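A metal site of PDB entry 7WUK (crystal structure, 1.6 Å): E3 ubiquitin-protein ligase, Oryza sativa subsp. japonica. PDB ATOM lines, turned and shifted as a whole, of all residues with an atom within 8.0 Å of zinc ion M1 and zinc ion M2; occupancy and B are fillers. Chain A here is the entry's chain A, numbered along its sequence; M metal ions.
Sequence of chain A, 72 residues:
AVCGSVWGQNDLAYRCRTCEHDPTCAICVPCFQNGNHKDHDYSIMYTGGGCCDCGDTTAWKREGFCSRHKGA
Of the 28 residues printed, 4 come within 4 Å of zinc ion M1. The nearest printed residue that does not touch zinc ion M1 is Ser 5 (4.1 Å).
Zinc ion M2 is bound by the side-chain sulfur of Cys 54 (2.3 Å), the side-chain sulfur of Cys 66 (2.3 Å) and the side-chain sulfur of Cys 31 (2.4 Å).
Merely in contact with zinc ion M2: His 69 (2.1 Å). Four residues have an atom within 4 Å of zinc ion M2: Cys 31, Cys 54, Cys 66 and His 69.
Zinc ion M1 is bound by SG of Cys 3. Zinc ion M1 is bound by SG of Cys 52. Zinc ion M1 is bound by SG of Cys 28 (2.3 Å). Zinc ion M1 is bound by SG of Cys 31, at 2.4 Å. Zinc ion M1 has four donor atoms within binding distance.
The side-chain sulfur (SG) of Cys 3 sits close to the backbone NH (N) of Ser 5, 3.4 Å away. N of Arg 68 lies close to SG of Cys 66 (3.4 Å). O of Ser 5 sits at hydrogen-bond distance from N of Cys 52, at 3.0 Å. N of His 69 lies close to SG of Cys 66, 3.7 Å away. NE2 of His 69 sits close to SG of Cys 31 (3.7 Å). The backbone NH (N) of Cys 54 lies close to the side-chain sulfur (SG) of Cys 52 (3.4 Å). N of Cys 3 lies within hydrogen-bond range of O of Cys 54 (2.9 Å).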
ATOM      1  N   VAL A   2     -10.626  11.535 -26.170  1.00  0.00           N
ATOM      2  CA  VAL A   2     -11.253  10.960 -24.897  1.00  0.00           C
ATOM      3  C   VAL A   2     -10.834  11.879 -23.737  1.00  0.00           C
ATOM      4  O   VAL A   2      -9.626  12.167 -23.586  1.00  0.00           O
ATOM      5  CB  VAL A   2     -10.809   9.520 -24.567  1.00  0.00           C
ATOM      6  CG1 VAL A   2     -11.220   9.087 -23.149  1.00  0.00           C
ATOM      7  CG2 VAL A   2     -11.346   8.501 -25.571  1.00  0.00           C
ATOM      8  N   CYS A   3     -11.789  12.271 -22.888  1.00  0.00           N
ATOM      9  CA  CYS A   3     -11.526  13.179 -21.760  1.00  0.00           C
ATOM     10  C   CYS A   3     -10.433  12.598 -20.864  1.00  0.00           C
ATOM     11  O   CYS A   3     -10.504  11.436 -20.469  1.00  0.00           O
ATOM     12  CB  CYS A   3     -12.795  13.392 -20.939  1.00  0.00           C
ATOM     13  SG  CYS A   3     -12.538  14.568 -19.583  1.00  0.00           S
ATOM     14  N   GLY A   4      -9.454  13.437 -20.528  1.00  0.00           N
ATOM     15  CA  GLY A   4      -8.317  13.081 -19.675  1.00  0.00           C
ATOM     16  C   GLY A   4      -8.549  13.353 -18.196  1.00  0.00           C
ATOM     17  O   GLY A   4      -7.608  13.190 -17.395  1.00  0.00           O
ATOM     18  N   SER A   5      -9.757  13.719 -17.796  1.00  0.00           N
ATOM     19  CA  SER A   5     -10.053  14.116 -16.399  1.00  0.00           C
ATOM     20  C   SER A   5      -9.914  12.931 -15.451  1.00  0.00           C
ATOM     21  O   SER A   5     -10.391  11.865 -15.787  1.00  0.00           O
ATOM     22  CB  SER A   5     -11.425  14.745 -16.277  1.00  0.00           C
ATOM     23  OG  SER A   5     -11.725  14.944 -14.910  1.00  0.00           O
ATOM     24  N   VAL A   6      -9.253  13.136 -14.322  1.00  0.00           N
ATOM     25  CA  VAL A   6      -9.192  12.135 -13.223  1.00  0.00           C
ATOM     26  C   VAL A   6      -9.741  12.840 -11.982  1.00  0.00           C
ATOM     27  O   VAL A   6      -9.519  14.053 -11.796  1.00  0.00           O
ATOM     28  CB  VAL A   6      -7.782  11.561 -13.012  1.00  0.00           C
ATOM     29  CG1 VAL A   6      -7.320  10.799 -14.264  1.00  0.00           C
ATOM     30  CG2 VAL A   6      -6.819  12.637 -12.581  1.00  0.00           C
ATOM     31  N   TRP A   7     -10.359  12.087 -11.108  1.00  0.00           N
ATOM     32  CA  TRP A   7     -10.852  12.627  -9.833  1.00  0.00           C
ATOM     33  C   TRP A   7     -10.731  11.589  -8.727  1.00  0.00           C
ATOM     34  O   TRP A   7     -10.465  10.406  -8.992  1.00  0.00           O
ATOM     35  CB  TRP A   7     -12.283  13.150  -9.970  1.00  0.00           C
ATOM     36  CG  TRP A   7     -13.298  12.077 -10.248  1.00  0.00           C
ATOM     37  CD1 TRP A   7     -14.008  11.358  -9.324  1.00  0.00           C
ATOM     38  CD2 TRP A   7     -13.780  11.621 -11.527  1.00  0.00           C
ATOM     39  NE1 TRP A   7     -14.858  10.498  -9.941  1.00  0.00           N
ATOM     40  CE2 TRP A   7     -14.733  10.616 -11.291  1.00  0.00           C
ATOM     41  CE3 TRP A   7     -13.496  11.964 -12.858  1.00  0.00           C
ATOM     42  CZ2 TRP A   7     -15.403   9.958 -12.303  1.00  0.00           C
ATOM     43  CZ3 TRP A   7     -14.222  11.355 -13.858  1.00  0.00           C
ATOM     44  CH2 TRP A   7     -15.107  10.329 -13.584  1.00  0.00           C
ATOM     45  N   ALA A  26     -18.590   6.400 -15.711  1.00  0.00           N
ATOM     46  CA  ALA A  26     -18.844   7.725 -15.136  1.00  0.00           C
ATOM     47  C   ALA A  26     -18.198   8.770 -16.012  1.00  0.00           C
ATOM     48  O   ALA A  26     -17.196   8.462 -16.677  1.00  0.00           O
ATOM     49  CB  ALA A  26     -18.322   7.849 -13.719  1.00  0.00           C
ATOM     50  N   ILE A  27     -18.754   9.973 -15.944  1.00  0.00           N
ATOM     51  CA  ILE A  27     -18.151  11.144 -16.634  1.00  0.00           C
ATOM     52  C   ILE A  27     -18.000  12.286 -15.648  1.00  0.00           C
ATOM     53  O   ILE A  27     -18.755  12.382 -14.683  1.00  0.00           O
ATOM     54  CB  ILE A  27     -18.880  11.596 -17.902  1.00  0.00           C
ATOM     55  CG1 ILE A  27     -20.310  12.076 -17.653  1.00  0.00           C
ATOM     56  CG2 ILE A  27     -18.840  10.480 -18.948  1.00  0.00           C
ATOM     57  CD1 ILE A  27     -20.930  12.699 -18.879  1.00  0.00           C
ATOM     58  N   CYS A  28     -17.041  13.146 -15.901  1.00  0.00           N
ATOM     59  CA  CYS A  28     -16.736  14.300 -15.028  1.00  0.00           C
ATOM     60  C   CYS A  28     -17.868  15.338 -15.100  1.00  0.00           C
ATOM     61  O   CYS A  28     -18.689  15.340 -16.011  1.00  0.00           O
ATOM     62  CB  CYS A  28     -15.350  14.861 -15.359  1.00  0.00           C
ATOM     63  SG  CYS A  28     -15.252  15.738 -16.943  1.00  0.00           S
ATOM     64  N   VAL A  29     -17.906  16.190 -14.091  1.00  0.00           N
ATOM     65  CA  VAL A  29     -19.002  17.176 -14.030  1.00  0.00           C
ATOM     66  C   VAL A  29     -18.987  18.018 -15.318  1.00  0.00           C
ATOM     67  O   VAL A  29     -20.012  18.201 -15.922  1.00  0.00           O
ATOM     68  CB  VAL A  29     -18.917  18.002 -12.740  1.00  0.00           C
ATOM     69  CG1 VAL A  29     -19.798  19.243 -12.861  1.00  0.00           C
ATOM     70  CG2 VAL A  29     -19.330  17.170 -11.535  1.00  0.00           C
ATOM     71  N   PRO A  30     -17.846  18.589 -15.773  1.00  0.00           N
ATOM     72  CA  PRO A  30     -17.898  19.408 -16.995  1.00  0.00           C
ATOM     73  C   PRO A  30     -18.359  18.660 -18.232  1.00  0.00           C
ATOM     74  O   PRO A  30     -19.088  19.201 -19.042  1.00  0.00           O
ATOM     75  CB  PRO A  30     -16.493  19.982 -17.128  1.00  0.00           C
ATOM     76  CG  PRO A  30     -15.845  19.813 -15.803  1.00  0.00           C
ATOM     77  CD  PRO A  30     -16.602  18.771 -15.030  1.00  0.00           C
ATOM     78  N   CYS A  31     -17.952  17.395 -18.382  1.00  0.00           N
ATOM     79  CA  CYS A  31     -18.418  16.627 -19.537  1.00  0.00           C
ATOM     80  C   CYS A  31     -19.932  16.419 -19.436  1.00  0.00           C
ATOM     81  O   CYS A  31     -20.583  16.562 -20.455  1.00  0.00           O
ATOM     82  CB  CYS A  31     -17.687  15.312 -19.623  1.00  0.00           C
ATOM     83  SG  CYS A  31     -16.007  15.577 -20.297  1.00  0.00           S
ATOM     84  N   PHE A  32     -20.470  16.178 -18.258  1.00  0.00           N
ATOM     85  CA  PHE A  32     -21.937  16.090 -18.083  1.00  0.00           C
ATOM     86  C   PHE A  32     -22.580  17.410 -18.500  1.00  0.00           C
ATOM     87  O   PHE A  32     -23.576  17.388 -19.280  1.00  0.00           O
ATOM     88  CB  PHE A  32     -22.315  15.711 -16.651  1.00  0.00           C
ATOM     89  CG  PHE A  32     -23.805  15.574 -16.546  1.00  0.00           C
ATOM     90  CD1 PHE A  32     -24.428  14.380 -16.900  1.00  0.00           C
ATOM     91  CD2 PHE A  32     -24.569  16.645 -16.154  1.00  0.00           C
ATOM     92  CE1 PHE A  32     -25.813  14.294 -16.881  1.00  0.00           C
ATOM     93  CE2 PHE A  32     -25.958  16.543 -16.075  1.00  0.00           C
ATOM     94  CZ  PHE A  32     -26.555  15.370 -16.459  1.00  0.00           C
ATOM     95  N   ASN A  34     -21.683  19.759 -20.381  1.00  0.00           N
ATOM     96  CA  ASN A  34     -21.480  20.151 -21.791  1.00  0.00           C
ATOM     97  C   ASN A  34     -22.108  19.137 -22.736  1.00  0.00           C
ATOM     98  O   ASN A  34     -21.873  19.235 -23.940  1.00  0.00           O
ATOM     99  CB  ASN A  34     -19.993  20.400 -22.063  1.00  0.00           C
ATOM    100  CG  ASN A  34     -19.507  21.691 -21.469  1.00  0.00           C
ATOM    101  OD1 ASN A  34     -18.367  21.793 -20.993  1.00  0.00           O
ATOM    102  ND2 ASN A  34     -20.324  22.721 -21.631  1.00  0.00           N
ATOM    103  N   GLY A  35     -22.855  18.152 -22.227  1.00  0.00           N
ATOM    104  CA  GLY A  35     -23.580  17.159 -23.032  1.00  0.00           C
ATOM    105  C   GLY A  35     -25.077  17.241 -22.823  1.00  0.00           C
ATOM    106  O   GLY A  35     -25.582  18.118 -22.086  1.00  0.00           O
ATOM    107  N   CYS A  51     -11.571   7.866 -13.733  1.00  0.00           N
ATOM    108  CA  CYS A  51     -11.160   8.545 -14.981  1.00  0.00           C
ATOM    109  C   CYS A  51     -12.430   8.755 -15.805  1.00  0.00           C
ATOM    110  O   CYS A  51     -13.316   7.943 -15.780  1.00  0.00           O
ATOM    111  CB  CYS A  51     -10.217   7.739 -15.861  1.00  0.00           C
ATOM    112  SG  CYS A  51      -8.625   7.427 -15.073  1.00  0.00           S
ATOM    113  N   CYS A  52     -12.495   9.838 -16.542  1.00  0.00           N
ATOM    114  CA  CYS A  52     -13.725  10.149 -17.299  1.00  0.00           C
ATOM    115  C   CYS A  52     -13.883   9.209 -18.498  1.00  0.00           C
ATOM    116  O   CYS A  52     -12.855   8.939 -19.181  1.00  0.00           O
ATOM    117  CB  CYS A  52     -13.643  11.585 -17.780  1.00  0.00           C
ATOM    118  SG  CYS A  52     -15.195  12.168 -18.500  1.00  0.00           S
ATOM    119  N   ASP A  53     -15.115   8.806 -18.802  1.00  0.00           N
ATOM    120  CA  ASP A  53     -15.450   7.908 -19.933  1.00  0.00           C
ATOM    121  C   ASP A  53     -15.912   8.714 -21.151  1.00  0.00           C
ATOM    122  O   ASP A  53     -16.246   8.067 -22.188  1.00  0.00           O
ATOM    123  CB  ASP A  53     -16.503   6.892 -19.509  1.00  0.00           C
ATOM    124  CG  ASP A  53     -15.891   5.847 -18.588  1.00  0.00           C
ATOM    125  OD1 ASP A  53     -14.709   5.505 -18.811  1.00  0.00           O
ATOM    126  OD2 ASP A  53     -16.552   5.418 -17.643  1.00  0.00           O
ATOM    127  N   CYS A  54     -15.990  10.044 -21.054  1.00  0.00           N
ATOM    128  CA  CYS A  54     -16.531  10.865 -22.175  1.00  0.00           C
ATOM    129  C   CYS A  54     -15.612  10.781 -23.394  1.00  0.00           C
ATOM    130  O   CYS A  54     -14.414  11.090 -23.276  1.00  0.00           O
ATOM    131  CB  CYS A  54     -16.645  12.306 -21.744  1.00  0.00           C
ATOM    132  SG  CYS A  54     -17.448  13.330 -22.989  1.00  0.00           S
ATOM    133  N   GLY A  55     -16.176  10.414 -24.525  1.00  0.00           N
ATOM    134  CA  GLY A  55     -15.380  10.202 -25.763  1.00  0.00           C
ATOM    135  C   GLY A  55     -14.988   8.775 -25.995  1.00  0.00           C
ATOM    136  O   GLY A  55     -14.570   8.476 -27.151  1.00  0.00           O
ATOM    137  N   ASP A  56     -15.101   7.893 -24.980  1.00  0.00           N
ATOM    138  CA  ASP A  56     -14.693   6.472 -25.057  1.00  0.00           C
ATOM    139  C   ASP A  56     -15.871   5.633 -25.553  1.00  0.00           C
ATOM    140  O   ASP A  56     -16.763   5.302 -24.736  1.00  0.00           O
ATOM    141  CB  ASP A  56     -14.195   5.965 -23.709  1.00  0.00           C
ATOM    142  CG  ASP A  56     -13.657   4.542 -23.773  1.00  0.00           C
ATOM    143  OD1 ASP A  56     -13.763   3.900 -24.854  1.00  0.00           O
ATOM    144  OD2 ASP A  56     -13.154   4.081 -22.707  1.00  0.00           O
ATOM    145  N   TRP A  60     -19.154   4.364 -23.242  1.00  0.00           N
ATOM    146  CA  TRP A  60     -20.208   5.407 -23.171  1.00  0.00           C
ATOM    147  C   TRP A  60     -20.837   5.573 -24.563  1.00  0.00           C
ATOM    148  O   TRP A  60     -20.103   5.662 -25.571  1.00  0.00           O
ATOM    149  CB  TRP A  60     -19.592   6.733 -22.727  1.00  0.00           C
ATOM    150  CG  TRP A  60     -20.499   7.737 -22.103  1.00  0.00           C
ATOM    151  CD1 TRP A  60     -21.024   8.839 -22.707  1.00  0.00           C
ATOM    152  CD2 TRP A  60     -20.936   7.778 -20.727  1.00  0.00           C
ATOM    153  NE1 TRP A  60     -21.713   9.593 -21.802  1.00  0.00           N
ATOM    154  CE2 TRP A  60     -21.701   8.957 -20.586  1.00  0.00           C
ATOM    155  CE3 TRP A  60     -20.770   6.948 -19.622  1.00  0.00           C
ATOM    156  CZ2 TRP A  60     -22.270   9.326 -19.386  1.00  0.00           C
ATOM    157  CZ3 TRP A  60     -21.374   7.301 -18.438  1.00  0.00           C
ATOM    158  CH2 TRP A  60     -22.117   8.477 -18.326  1.00  0.00           C
ATOM    159  N   GLY A  64     -24.103  10.566 -25.806  1.00  0.00           N
ATOM    160  CA  GLY A  64     -23.817  11.078 -24.465  1.00  0.00           C
ATOM    161  C   GLY A  64     -22.460  11.753 -24.357  1.00  0.00           C
ATOM    162  O   GLY A  64     -22.142  12.143 -23.261  1.00  0.00           O
ATOM    163  N   PHE A  65     -21.719  11.924 -25.451  1.00  0.00           N
ATOM    164  CA  PHE A  65     -20.435  12.651 -25.426  1.00  0.00           C
ATOM    165  C   PHE A  65     -20.708  14.144 -25.319  1.00  0.00           C
ATOM    166  O   PHE A  65     -21.690  14.671 -25.983  1.00  0.00           O
ATOM    167  CB  PHE A  65     -19.597  12.384 -26.685  1.00  0.00           C
ATOM    168  CG  PHE A  65     -19.094  10.982 -26.875  1.00  0.00           C
ATOM    169  CD1 PHE A  65     -19.238  10.006 -25.901  1.00  0.00           C
ATOM    170  CD2 PHE A  65     -18.476  10.618 -28.061  1.00  0.00           C
ATOM    171  CE1 PHE A  65     -18.767   8.720 -26.104  1.00  0.00           C
ATOM    172  CE2 PHE A  65     -17.987   9.334 -28.247  1.00  0.00           C
ATOM    173  CZ  PHE A  65     -18.124   8.386 -27.260  1.00  0.00           C
ATOM    174  N   CYS A  66     -19.867  14.857 -24.590  1.00  0.00           N
ATOM    175  CA  CYS A  66     -19.991  16.342 -24.566  1.00  0.00           C
ATOM    176  C   CYS A  66     -19.518  16.959 -25.878  1.00  0.00           C
ATOM    177  O   CYS A  66     -18.949  16.288 -26.737  1.00  0.00           O
ATOM    178  CB  CYS A  66     -19.295  16.954 -23.359  1.00  0.00           C
ATOM    179  SG  CYS A  66     -17.495  17.102 -23.580  1.00  0.00           S
ATOM    180  N   SER A  67     -19.797  18.248 -26.005  1.00  0.00           N
ATOM    181  CA  SER A  67     -19.472  19.055 -27.198  1.00  0.00           C
ATOM    182  C   SER A  67     -17.969  18.964 -27.483  1.00  0.00           C
ATOM    183  O   SER A  67     -17.568  19.055 -28.646  1.00  0.00           O
ATOM    184  CB  SER A  67     -19.957  20.458 -26.991  1.00  0.00           C
ATOM    185  OG  SER A  67     -19.487  20.995 -25.761  1.00  0.00           O
ATOM    186  N   ARG A  68     -17.138  18.791 -26.460  1.00  0.00           N
ATOM    187  CA  ARG A  68     -15.662  18.942 -26.534  1.00  0.00           C
ATOM    188  C   ARG A  68     -14.994  17.604 -26.877  1.00  0.00           C
ATOM    189  O   ARG A  68     -13.839  17.654 -27.326  1.00  0.00           O
ATOM    190  CB  ARG A  68     -15.211  19.605 -25.223  1.00  0.00           C
ATOM    191  CG  ARG A  68     -16.010  20.862 -24.878  1.00  0.00           C
ATOM    192  CD  ARG A  68     -15.575  21.598 -23.605  1.00  0.00           C
ATOM    193  NE  ARG A  68     -14.191  22.022 -23.715  1.00  0.00           N
ATOM    194  CZ  ARG A  68     -13.146  21.342 -23.267  1.00  0.00           C
ATOM    195  NH1 ARG A  68     -13.311  20.205 -22.611  1.00  0.00           N
ATOM    196  NH2 ARG A  68     -11.932  21.782 -23.504  1.00  0.00           N
ATOM    197  N   HIS A  69     -15.660  16.436 -26.734  1.00  0.00           N
ATOM    198  CA  HIS A  69     -15.065  15.096 -27.008  1.00  0.00           C
ATOM    199  C   HIS A  69     -16.005  14.220 -27.861  1.00  0.00           C
ATOM    200  O   HIS A  69     -16.608  14.773 -28.767  1.00  0.00           O
ATOM    201  CB  HIS A  69     -14.730  14.328 -25.714  1.00  0.00           C
ATOM    202  CG  HIS A  69     -14.045  15.128 -24.661  1.00  0.00           C
ATOM    203  ND1 HIS A  69     -12.697  15.545 -24.726  1.00  0.00           N
ATOM    204  CD2 HIS A  69     -14.492  15.558 -23.470  1.00  0.00           C
ATOM    205  CE1 HIS A  69     -12.412  16.268 -23.663  1.00  0.00           C
ATOM    206  NE2 HIS A  69     -13.483  16.256 -22.868  1.00  0.00           N
HETATM  207 ZN    ZN M   1     -14.650  14.405 -18.752  1.00  0.00          ZN
HETATM  208 ZN    ZN M   2     -16.407  15.314 -22.665  1.00  0.00          ZN
